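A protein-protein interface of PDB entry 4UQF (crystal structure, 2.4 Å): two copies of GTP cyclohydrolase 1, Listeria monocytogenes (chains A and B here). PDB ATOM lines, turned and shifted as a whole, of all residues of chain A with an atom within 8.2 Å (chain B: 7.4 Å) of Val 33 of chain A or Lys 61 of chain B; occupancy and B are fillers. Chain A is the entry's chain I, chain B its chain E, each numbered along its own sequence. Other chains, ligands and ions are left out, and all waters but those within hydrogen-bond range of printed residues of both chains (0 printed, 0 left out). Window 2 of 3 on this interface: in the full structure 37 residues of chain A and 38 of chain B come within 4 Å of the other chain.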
ATOM      1  N   VAL A  26      21.397  24.499 -15.321  1.00  0.00           N
ATOM      2  CA  VAL A  26      21.208  23.065 -15.209  1.00  0.00           C
ATOM      3  C   VAL A  26      21.917  22.533 -13.983  1.00  0.00           C
ATOM      4  O   VAL A  26      21.384  21.675 -13.263  1.00  0.00           O
ATOM      5  CB  VAL A  26      21.677  22.327 -16.472  1.00  0.00           C
ATOM      6  CG1 VAL A  26      21.669  20.816 -16.258  1.00  0.00           C
ATOM      7  CG2 VAL A  26      20.755  22.676 -17.635  1.00  0.00           C
ATOM      8  N   LYS A  27      23.107  23.033 -13.717  1.00  0.00           N
ATOM      9  CA  LYS A  27      23.850  22.588 -12.530  1.00  0.00           C
ATOM     10  C   LYS A  27      23.099  22.919 -11.248  1.00  0.00           C
ATOM     11  O   LYS A  27      22.990  22.096 -10.346  1.00  0.00           O
ATOM     12  CB  LYS A  27      25.230  23.220 -12.501  1.00  0.00           C
ATOM     13  CG  LYS A  27      26.065  22.718 -11.350  1.00  0.00           C
ATOM     14  CD  LYS A  27      27.558  22.949 -11.532  1.00  0.00           C
ATOM     15  CE  LYS A  27      28.258  22.584 -10.231  1.00  0.00           C
ATOM     16  NZ  LYS A  27      29.718  22.822 -10.261  1.00  0.00           N
ATOM     17  N   VAL A  28      22.533  24.116 -11.197  1.00  0.00           N
ATOM     18  CA  VAL A  28      21.691  24.498 -10.079  1.00  0.00           C
ATOM     19  C   VAL A  28      20.514  23.528  -9.918  1.00  0.00           C
ATOM     20  O   VAL A  28      20.175  23.104  -8.816  1.00  0.00           O
ATOM     21  CB  VAL A  28      21.162  25.937 -10.273  1.00  0.00           C
ATOM     22  CG1 VAL A  28      20.031  26.239  -9.291  1.00  0.00           C
ATOM     23  CG2 VAL A  28      22.296  26.929 -10.130  1.00  0.00           C
ATOM     24  N   ILE A  29      19.885  23.176 -11.032  1.00  0.00           N
ATOM     25  CA  ILE A  29      18.760  22.241 -10.998  1.00  0.00           C
ATOM     26  C   ILE A  29      19.163  20.884 -10.424  1.00  0.00           C
ATOM     27  O   ILE A  29      18.476  20.334  -9.566  1.00  0.00           O
ATOM     28  CB  ILE A  29      18.158  22.094 -12.396  1.00  0.00           C
ATOM     29  CG1 ILE A  29      17.436  23.396 -12.763  1.00  0.00           C
ATOM     30  CG2 ILE A  29      17.175  20.949 -12.426  1.00  0.00           C
ATOM     31  CD1 ILE A  29      16.995  23.505 -14.206  1.00  0.00           C
ATOM     32  N   LEU A  30      20.306  20.367 -10.872  1.00  0.00           N
ATOM     33  CA  LEU A  30      20.808  19.114 -10.357  1.00  0.00           C
ATOM     34  C   LEU A  30      21.076  19.136  -8.852  1.00  0.00           C
ATOM     35  O   LEU A  30      20.791  18.170  -8.161  1.00  0.00           O
ATOM     36  CB  LEU A  30      22.093  18.713 -11.096  1.00  0.00           C
ATOM     37  CG  LEU A  30      21.910  18.379 -12.571  1.00  0.00           C
ATOM     38  CD1 LEU A  30      23.258  18.286 -13.247  1.00  0.00           C
ATOM     39  CD2 LEU A  30      21.120  17.093 -12.744  1.00  0.00           C
ATOM     40  N   GLU A  31      21.673  20.208  -8.358  1.00  0.00           N
ATOM     41  CA  GLU A  31      21.892  20.323  -6.915  1.00  0.00           C
ATOM     42  C   GLU A  31      20.538  20.350  -6.235  1.00  0.00           C
ATOM     43  O   GLU A  31      20.310  19.621  -5.276  1.00  0.00           O
ATOM     44  CB  GLU A  31      22.695  21.580  -6.532  1.00  0.00           C
ATOM     45  CG  GLU A  31      24.109  21.562  -7.116  1.00  0.00           C
ATOM     46  CD  GLU A  31      24.891  22.863  -6.983  1.00  0.00           C
ATOM     47  OE1 GLU A  31      24.283  23.959  -7.019  1.00  0.00           O
ATOM     48  OE2 GLU A  31      26.139  22.790  -6.899  1.00  0.00           O
ATOM     49  N   ALA A  32      19.626  21.157  -6.760  1.00  0.00           N
ATOM     50  CA  ALA A  32      18.338  21.362  -6.114  1.00  0.00           C
ATOM     51  C   ALA A  32      17.515  20.080  -6.007  1.00  0.00           C
ATOM     52  O   ALA A  32      16.761  19.929  -5.062  1.00  0.00           O
ATOM     53  CB  ALA A  32      17.556  22.425  -6.851  1.00  0.00           C
ATOM     54  N   VAL A  33      17.656  19.154  -6.966  1.00  0.00           N
ATOM     55  CA  VAL A  33      16.879  17.919  -6.896  1.00  0.00           C
ATOM     56  C   VAL A  33      17.538  16.865  -6.009  1.00  0.00           C
ATOM     57  O   VAL A  33      16.944  15.831  -5.739  1.00  0.00           O
ATOM     58  CB  VAL A  33      16.570  17.300  -8.281  1.00  0.00           C
ATOM     59  CG1 VAL A  33      15.792  18.276  -9.139  1.00  0.00           C
ATOM     60  CG2 VAL A  33      17.843  16.828  -8.983  1.00  0.00           C
ATOM     61  N   GLY A  34      18.745  17.129  -5.534  1.00  0.00           N
ATOM     62  CA  GLY A  34      19.374  16.264  -4.540  1.00  0.00           C
ATOM     63  C   GLY A  34      20.398  15.362  -5.169  1.00  0.00           C
ATOM     64  O   GLY A  34      20.740  14.320  -4.624  1.00  0.00           O
ATOM     65  N   GLU A  35      20.889  15.755  -6.330  1.00  0.00           N
ATOM     66  CA  GLU A  35      21.831  14.943  -7.051  1.00  0.00           C
ATOM     67  C   GLU A  35      23.222  15.483  -6.759  1.00  0.00           C
ATOM     68  O   GLU A  35      23.378  16.562  -6.207  1.00  0.00           O
ATOM     69  CB  GLU A  35      21.474  15.040  -8.523  1.00  0.00           C
ATOM     70  CG  GLU A  35      22.193  14.157  -9.487  1.00  0.00           C
ATOM     71  CD  GLU A  35      22.146  12.681  -9.223  1.00  0.00           C
ATOM     72  OE1 GLU A  35      23.010  12.194  -8.467  1.00  0.00           O
ATOM     73  OE2 GLU A  35      21.319  11.992  -9.835  1.00  0.00           O
ATOM     74  N   ASN A  36      24.243  14.694  -7.063  1.00  0.00           N
ATOM     75  CA  ASN A  36      25.623  15.139  -6.931  1.00  0.00           C
ATOM     76  C   ASN A  36      26.189  15.545  -8.286  1.00  0.00           C
ATOM     77  O   ASN A  36      26.607  14.685  -9.075  1.00  0.00           O
ATOM     78  CB  ASN A  36      26.476  14.034  -6.323  1.00  0.00           C
ATOM     79  CG  ASN A  36      27.947  14.379  -6.309  1.00  0.00           C
ATOM     80  OD1 ASN A  36      28.367  15.498  -6.652  1.00  0.00           O
ATOM     81  ND2 ASN A  36      28.751  13.409  -5.940  1.00  0.00           N
ATOM     82  N   LEU A  42      27.300  12.920 -14.329  1.00  0.00           N
ATOM     83  CA  LEU A  42      26.680  14.235 -14.473  1.00  0.00           C
ATOM     84  C   LEU A  42      27.624  15.369 -14.821  1.00  0.00           C
ATOM     85  O   LEU A  42      27.165  16.464 -15.149  1.00  0.00           O
ATOM     86  CB  LEU A  42      25.925  14.588 -13.204  1.00  0.00           C
ATOM     87  CG  LEU A  42      24.732  13.683 -12.984  1.00  0.00           C
ATOM     88  CD1 LEU A  42      24.111  14.016 -11.659  1.00  0.00           C
ATOM     89  CD2 LEU A  42      23.689  13.790 -14.086  1.00  0.00           C
ATOM     90  N   GLN B  16      12.030  16.992   0.563  1.00  0.00           N
ATOM     91  CA  GLN B  16      11.337  18.213   0.043  1.00  0.00           C
ATOM     92  C   GLN B  16      12.417  18.991  -0.757  1.00  0.00           C
ATOM     93  O   GLN B  16      13.407  19.472  -0.182  1.00  0.00           O
ATOM     94  CB  GLN B  16      10.696  19.042   1.245  1.00  0.00           C
ATOM     95  CG  GLN B  16       9.277  19.744   1.128  1.00  0.00           C
ATOM     96  CD  GLN B  16       8.779  19.868  -0.263  1.00  0.00           C
ATOM     97  OE1 GLN B  16       7.963  19.067  -0.745  1.00  0.00           O
ATOM     98  NE2 GLN B  16       9.238  20.882  -0.904  1.00  0.00           N
ATOM     99  N   ILE B  17      12.264  19.078  -2.089  1.00  0.00           N
ATOM    100  CA  ILE B  17      13.294  19.730  -2.915  1.00  0.00           C
ATOM    101  C   ILE B  17      12.884  21.177  -3.099  1.00  0.00           C
ATOM    102  O   ILE B  17      11.721  21.557  -2.919  1.00  0.00           O
ATOM    103  CB  ILE B  17      13.541  19.088  -4.302  1.00  0.00           C
ATOM    104  CG1 ILE B  17      12.302  19.289  -5.186  1.00  0.00           C
ATOM    105  CG2 ILE B  17      13.951  17.637  -4.135  1.00  0.00           C
ATOM    106  CD1 ILE B  17      12.209  18.612  -6.531  1.00  0.00           C
ATOM    107  N   ASP B  18      13.854  21.993  -3.453  1.00  0.00           N
ATOM    108  CA  ASP B  18      13.611  23.410  -3.572  1.00  0.00           C
ATOM    109  C   ASP B  18      13.063  23.734  -4.966  1.00  0.00           C
ATOM    110  O   ASP B  18      13.807  24.071  -5.886  1.00  0.00           O
ATOM    111  CB  ASP B  18      14.894  24.175  -3.281  1.00  0.00           C
ATOM    112  CG  ASP B  18      14.674  25.662  -3.183  1.00  0.00           C
ATOM    113  OD1 ASP B  18      13.558  26.143  -3.501  1.00  0.00           O
ATOM    114  OD2 ASP B  18      15.629  26.355  -2.782  1.00  0.00           O
ATOM    115  N   LYS B  21      13.804  27.283  -6.537  1.00  0.00           N
ATOM    116  CA  LYS B  21      15.147  27.360  -7.110  1.00  0.00           C
ATOM    117  C   LYS B  21      15.165  26.748  -8.516  1.00  0.00           C
ATOM    118  O   LYS B  21      15.761  27.314  -9.444  1.00  0.00           O
ATOM    119  CB  LYS B  21      16.140  26.646  -6.201  1.00  0.00           C
ATOM    120  CG  LYS B  21      17.592  26.986  -6.447  1.00  0.00           C
ATOM    121  CD  LYS B  21      18.507  26.128  -5.575  1.00  0.00           C
ATOM    122  CE  LYS B  21      18.859  26.841  -4.266  1.00  0.00           C
ATOM    123  NZ  LYS B  21      20.123  27.622  -4.389  1.00  0.00           N
ATOM    124  N   ILE B  22      14.506  25.608  -8.672  1.00  0.00           N
ATOM    125  CA  ILE B  22      14.464  24.941  -9.961  1.00  0.00           C
ATOM    126  C   ILE B  22      13.708  25.808 -10.956  1.00  0.00           C
ATOM    127  O   ILE B  22      14.143  25.990 -12.102  1.00  0.00           O
ATOM    128  CB  ILE B  22      13.793  23.572  -9.853  1.00  0.00           C
ATOM    129  CG1 ILE B  22      14.703  22.615  -9.098  1.00  0.00           C
ATOM    130  CG2 ILE B  22      13.486  23.010 -11.237  1.00  0.00           C
ATOM    131  CD1 ILE B  22      13.986  21.384  -8.584  1.00  0.00           C
ATOM    132  N   VAL B  49       7.769  22.301 -14.470  1.00  0.00           N
ATOM    133  CA  VAL B  49       8.971  21.512 -14.621  1.00  0.00           C
ATOM    134  C   VAL B  49       9.493  21.133 -13.242  1.00  0.00           C
ATOM    135  O   VAL B  49       9.967  20.014 -13.040  1.00  0.00           O
ATOM    136  CB  VAL B  49      10.035  22.246 -15.478  1.00  0.00           C
ATOM    137  CG1 VAL B  49      11.359  21.508 -15.459  1.00  0.00           C
ATOM    138  CG2 VAL B  49       9.541  22.375 -16.919  1.00  0.00           C
ATOM    139  N   ALA B  50       9.427  22.058 -12.303  1.00  0.00           N
ATOM    140  CA  ALA B  50       9.906  21.752 -10.963  1.00  0.00           C
ATOM    141  C   ALA B  50       9.113  20.596 -10.363  1.00  0.00           C
ATOM    142  O   ALA B  50       9.692  19.672  -9.807  1.00  0.00           O
ATOM    143  CB  ALA B  50       9.856  22.987 -10.061  1.00  0.00           C
ATOM    144  N   TYR B  53      10.062  17.344 -11.977  1.00  0.00           N
ATOM    145  CA  TYR B  53      11.322  16.813 -11.494  1.00  0.00           C
ATOM    146  C   TYR B  53      11.169  16.204 -10.111  1.00  0.00           C
ATOM    147  O   TYR B  53      11.735  15.152  -9.813  1.00  0.00           O
ATOM    148  CB  TYR B  53      12.405  17.879 -11.482  1.00  0.00           C
ATOM    149  CG  TYR B  53      13.015  18.182 -12.841  1.00  0.00           C
ATOM    150  CD1 TYR B  53      12.991  17.259 -13.863  1.00  0.00           C
ATOM    151  CD2 TYR B  53      13.641  19.385 -13.088  1.00  0.00           C
ATOM    152  CE1 TYR B  53      13.552  17.546 -15.087  1.00  0.00           C
ATOM    153  CE2 TYR B  53      14.198  19.680 -14.322  1.00  0.00           C
ATOM    154  CZ  TYR B  53      14.162  18.752 -15.320  1.00  0.00           C
ATOM    155  OH  TYR B  53      14.736  19.030 -16.558  1.00  0.00           O
ATOM    156  N   GLU B  54      10.354  16.832  -9.277  1.00  0.00           N
ATOM    157  CA  GLU B  54      10.098  16.276  -7.972  1.00  0.00           C
ATOM    158  C   GLU B  54       9.541  14.866  -8.075  1.00  0.00           C
ATOM    159  O   GLU B  54       9.904  13.964  -7.312  1.00  0.00           O
ATOM    160  CB  GLU B  54       9.137  17.179  -7.221  1.00  0.00           C
ATOM    161  CG  GLU B  54       8.809  16.722  -5.815  1.00  0.00           C
ATOM    162  CD  GLU B  54       8.121  17.820  -5.045  1.00  0.00           C
ATOM    163  OE1 GLU B  54       7.005  18.205  -5.447  1.00  0.00           O
ATOM    164  OE2 GLU B  54       8.693  18.318  -4.059  1.00  0.00           O
ATOM    165  N   PHE B  57      12.173  12.303 -10.222  1.00  0.00           N
ATOM    166  CA  PHE B  57      13.415  12.043  -9.519  1.00  0.00           C
ATOM    167  C   PHE B  57      13.184  11.705  -8.068  1.00  0.00           C
ATOM    168  O   PHE B  57      14.112  11.665  -7.300  1.00  0.00           O
ATOM    169  CB  PHE B  57      14.367  13.237  -9.627  1.00  0.00           C
ATOM    170  CG  PHE B  57      14.819  13.526 -11.030  1.00  0.00           C
ATOM    171  CD1 PHE B  57      14.994  12.489 -11.952  1.00  0.00           C
ATOM    172  CD2 PHE B  57      15.080  14.822 -11.434  1.00  0.00           C
ATOM    173  CE1 PHE B  57      15.422  12.750 -13.238  1.00  0.00           C
ATOM    174  CE2 PHE B  57      15.504  15.091 -12.719  1.00  0.00           C
ATOM    175  CZ  PHE B  57      15.682  14.049 -13.624  1.00  0.00           C
ATOM    176  N   ALA B  58      11.973  11.315  -7.719  1.00  0.00           N
ATOM    177  CA  ALA B  58      11.670  10.935  -6.332  1.00  0.00           C
ATOM    178  C   ALA B  58      12.532   9.759  -5.812  1.00  0.00           C
ATOM    179  O   ALA B  58      12.777   9.654  -4.619  1.00  0.00           O
ATOM    180  CB  ALA B  58      10.199  10.589  -6.216  1.00  0.00           C
ATOM    181  N   GLY B  59      12.985   8.885  -6.715  1.00  0.00           N
ATOM    182  CA  GLY B  59      13.811   7.714  -6.369  1.00  0.00           C
ATOM    183  C   GLY B  59      15.141   8.068  -5.710  1.00  0.00           C
ATOM    184  O   GLY B  59      15.713   7.254  -5.001  1.00  0.00           O
ATOM    185  N   LEU B  60      15.606   9.299  -5.912  1.00  0.00           N
ATOM    186  CA  LEU B  60      16.782   9.815  -5.207  1.00  0.00           C
ATOM    187  C   LEU B  60      16.621   9.785  -3.703  1.00  0.00           C
ATOM    188  O   LEU B  60      17.602   9.820  -2.995  1.00  0.00           O
ATOM    189  CB  LEU B  60      17.090  11.269  -5.632  1.00  0.00           C
ATOM    190  CG  LEU B  60      17.611  11.447  -7.055  1.00  0.00           C
ATOM    191  CD1 LEU B  60      17.637  12.916  -7.441  1.00  0.00           C
ATOM    192  CD2 LEU B  60      18.998  10.833  -7.204  1.00  0.00           C
ATOM    193  N   LYS B  61      15.383   9.766  -3.214  1.00  0.00           N
ATOM    194  CA  LYS B  61      15.104   9.782  -1.758  1.00  0.00           C
ATOM    195  C   LYS B  61      14.653   8.462  -1.200  1.00  0.00           C
ATOM    196  O   LYS B  61      14.281   8.382  -0.057  1.00  0.00           O
ATOM    197  CB  LYS B  61      14.056  10.835  -1.493  1.00  0.00           C
ATOM    198  CG  LYS B  61      14.584  12.038  -2.283  1.00  0.00           C
ATOM    199  CD  LYS B  61      14.690  13.302  -1.477  1.00  0.00           C
ATOM    200  CE  LYS B  61      15.097  14.495  -2.415  1.00  0.00           C
ATOM    201  NZ  LYS B  61      16.328  15.211  -1.942  1.00  0.00           N
ATOM    202  N   LYS B  62      14.672   7.422  -2.012  1.00  0.00           N
ATOM    203  CA  LYS B  62      14.157   6.142  -1.573  1.00  0.00           C
ATOM    204  C   LYS B  62      15.164   5.035  -1.761  1.00  0.00           C
ATOM    205  O   LYS B  62      15.948   5.067  -2.703  1.00  0.00           O
ATOM    206  CB  LYS B  62      12.874   5.844  -2.320  1.00  0.00           C
ATOM    207  N   ASP B  63      15.136   4.063  -0.857  1.00  0.00           N
ATOM    208  CA  ASP B  63      15.848   2.815  -1.067  1.00  0.00           C
ATOM    209  C   ASP B  63      14.904   1.857  -1.827  1.00  0.00           C
ATOM    210  O   ASP B  63      13.882   1.437  -1.290  1.00  0.00           O
ATOM    211  CB  ASP B  63      16.300   2.224   0.266  1.00  0.00           C
ATOM    212  CG  ASP B  63      17.078   0.913   0.108  1.00  0.00           C
ATOM    213  OD1 ASP B  63      17.348   0.475  -1.025  1.00  0.00           O
ATOM    214  OD2 ASP B  63      17.413   0.305   1.135  1.00  0.00           O
ATOM    215  N   PRO B  64      15.247   1.510  -3.080  1.00  0.00           N
ATOM    216  CA  PRO B  64      14.372   0.642  -3.879  1.00  0.00           C
ATOM    217  C   PRO B  64      14.311  -0.816  -3.395  1.00  0.00           C
ATOM    218  O   PRO B  64      13.369  -1.538  -3.744  1.00  0.00           O
ATOM    219  CB  PRO B  64      14.969   0.708  -5.284  1.00  0.00           C
ATOM    220  CG  PRO B  64      16.266   1.425  -5.169  1.00  0.00           C
ATOM    221  CD  PRO B  64      16.488   1.877  -3.781  1.00  0.00           C
ATOM    222  N   LEU B  95      18.998  14.592 -19.541  1.00  0.00           N
ATOM    223  CA  LEU B  95      17.760  14.768 -18.794  1.00  0.00           C
ATOM    224  C   LEU B  95      16.541  14.719 -19.681  1.00  0.00           C
ATOM    225  O   LEU B  95      15.610  15.495 -19.528  1.00  0.00           O
ATOM    226  CB  LEU B  95      17.791  16.064 -17.992  1.00  0.00           C
ATOM    227  CG  LEU B  95      18.965  16.197 -17.030  1.00  0.00           C
ATOM    228  CD1 LEU B  95      18.885  17.537 -16.345  1.00  0.00           C
ATOM    229  CD2 LEU B  95      18.983  15.079 -15.996  1.00  0.00           C
ATOM    230  N   ARG B 128      13.316   6.020 -11.166  1.00  0.00           N
ATOM    231  CA  ARG B 128      12.923   7.400 -10.844  1.00  0.00           C
ATOM    232  C   ARG B 128      14.108   8.244 -10.340  1.00  0.00           C
ATOM    233  O   ARG B 128      14.121   8.760  -9.222  1.00  0.00           O
ATOM    234  CB  ARG B 128      11.738   7.418  -9.845  1.00  0.00           C
ATOM    235  CG  ARG B 128      10.384   7.577 -10.538  1.00  0.00           C
ATOM    236  CD  ARG B 128       9.165   7.775  -9.603  1.00  0.00           C
ATOM    237  NE  ARG B 128       8.174   6.704  -9.415  1.00  0.00           N
ATOM    238  CZ  ARG B 128       8.323   5.640  -8.644  1.00  0.00           C
ATOM    239  NH1 ARG B 128       9.451   5.445  -7.984  1.00  0.00           N
ATOM    240  NH2 ARG B 128       7.343   4.756  -8.555  1.00  0.00           N
ATOM    241  N   ARG B 129      15.115   8.378 -11.197  1.00  0.00           N
ATOM    242  CA  ARG B 129      16.270   9.219 -10.933  1.00  0.00           C
ATOM    243  C   ARG B 129      17.032   9.306 -12.234  1.00  0.00           C
ATOM    244  O   ARG B 129      16.817   8.481 -13.107  1.00  0.00           O
ATOM    245  CB  ARG B 129      17.150   8.603  -9.864  1.00  0.00           C
ATOM    246  CG  ARG B 129      17.431   7.137 -10.103  1.00  0.00           C
ATOM    247  CD  ARG B 129      18.608   6.704  -9.279  1.00  0.00           C
ATOM    248  NE  ARG B 129      18.221   6.441  -7.902  1.00  0.00           N
ATOM    249  CZ  ARG B 129      19.008   6.621  -6.843  1.00  0.00           C
ATOM    250  NH1 ARG B 129      20.246   7.109  -6.970  1.00  0.00           N
ATOM    251  NH2 ARG B 129      18.542   6.332  -5.648  1.00  0.00           N
ATOM    252  N   PRO B 130      17.926  10.290 -12.375  1.00  0.00           N
ATOM    253  CA  PRO B 130      18.705  10.322 -13.597  1.00  0.00           C
ATOM    254  C   PRO B 130      19.460   9.031 -13.728  1.00  0.00           C
ATOM    255  O   PRO B 130      20.152   8.649 -12.799  1.00  0.00           O
ATOM    256  CB  PRO B 130      19.671  11.495 -13.385  1.00  0.00           C
ATOM    257  CG  PRO B 130      18.979  12.339 -12.366  1.00  0.00           C
ATOM    258  CD  PRO B 130      18.306  11.359 -11.453  1.00  0.00           C
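N of Lys 21 of chain B sits at hydrogen-bond distance from OD1 of Asp 18 of chain B (3.3 Å). The backbone NH (N) of Glu 35 of chain A is in hydrogen-bond range of the backbone carbonyl oxygen (O) of Leu 30 of chain A (3.0 Å).
Lys 21 of chain B touches Val 28 of chain A. Ile 17 of chain B touches Ala 32 of chain A (CB to O, 3.4 Å). Asp 18 of chain B touches Ala 32 of chain A (N to O, 3.9 Å). Ala 32 of chain A touches Ile 22 of chain B. Ile 17 of chain B touches Val 33 of chain A (CG2 to O, 3.8 Å). Val 33 of chain A touches Ile 22 of chain B (CG1 to CD1, 3.6 Å). Leu 60 of chain B touches Val 33 of chain A (CD1 to O, 3.4 Å). Val 33 of chain A touches Lys 61 of chain B (O to NZ, 3.9 Å). OE2 of Glu 35 of chain A touches CD2 of Leu 60 of chain B, 3.7 Å away. Pro 130 of chain B touches Glu 35 of chain A (CG to OE2, 3.5 Å).
Val 33 of chain A touches four residues of chain B. Lys 61 of chain B touches one residue of chain A. No residue of chain A comes within 4 Å of Lys 62 of chain B. Of the printed residues of chain A, Asp 18 of chain B touches Ala 32 (3.9 Å). Of the printed residues of chain A, Lys 21 of chain B touches Val 28 (3.8 Å). Of the printed residues of chain A, Ile 22 of chain B touches Ala 32 and Val 33. Printed residues of chain A within 4 Å of Pro 130 of chain B: Glu 35. The nearest residue of chain B that does not touch Val 33 of chain A is Tyr 53 of chain B (4.1 Å).
Of the 12 printed residues of chain A, 5 touch a printed residue of chain B. Printed residues of chain A that touch a printed residue of chain B: Val 28, Ile 29, Ala 32, Val 33 and Glu 35. Hydrophobic or aromatic side chains of chain A within 4 Å of the printed part of chain B: Val 28, Ile 29, Ala 32 and Val 33. Of the 21 printed residues of chain B, 8 touch a printed residue of chain A. Printed residues of chain B that touch a printed residue of chain A: Ile 17, Asp 18, Lys 21, Ile 22, Tyr 53, Leu 60, Lys 61 and Pro 130. Among the printed residues, 11 pairs touch across the chains. Among the printed residues, no Asp or Glu carboxylate lies within 4 Å of a Lys or Arg side-chain nitrogen of the other chain.
No position is printed for both chains.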
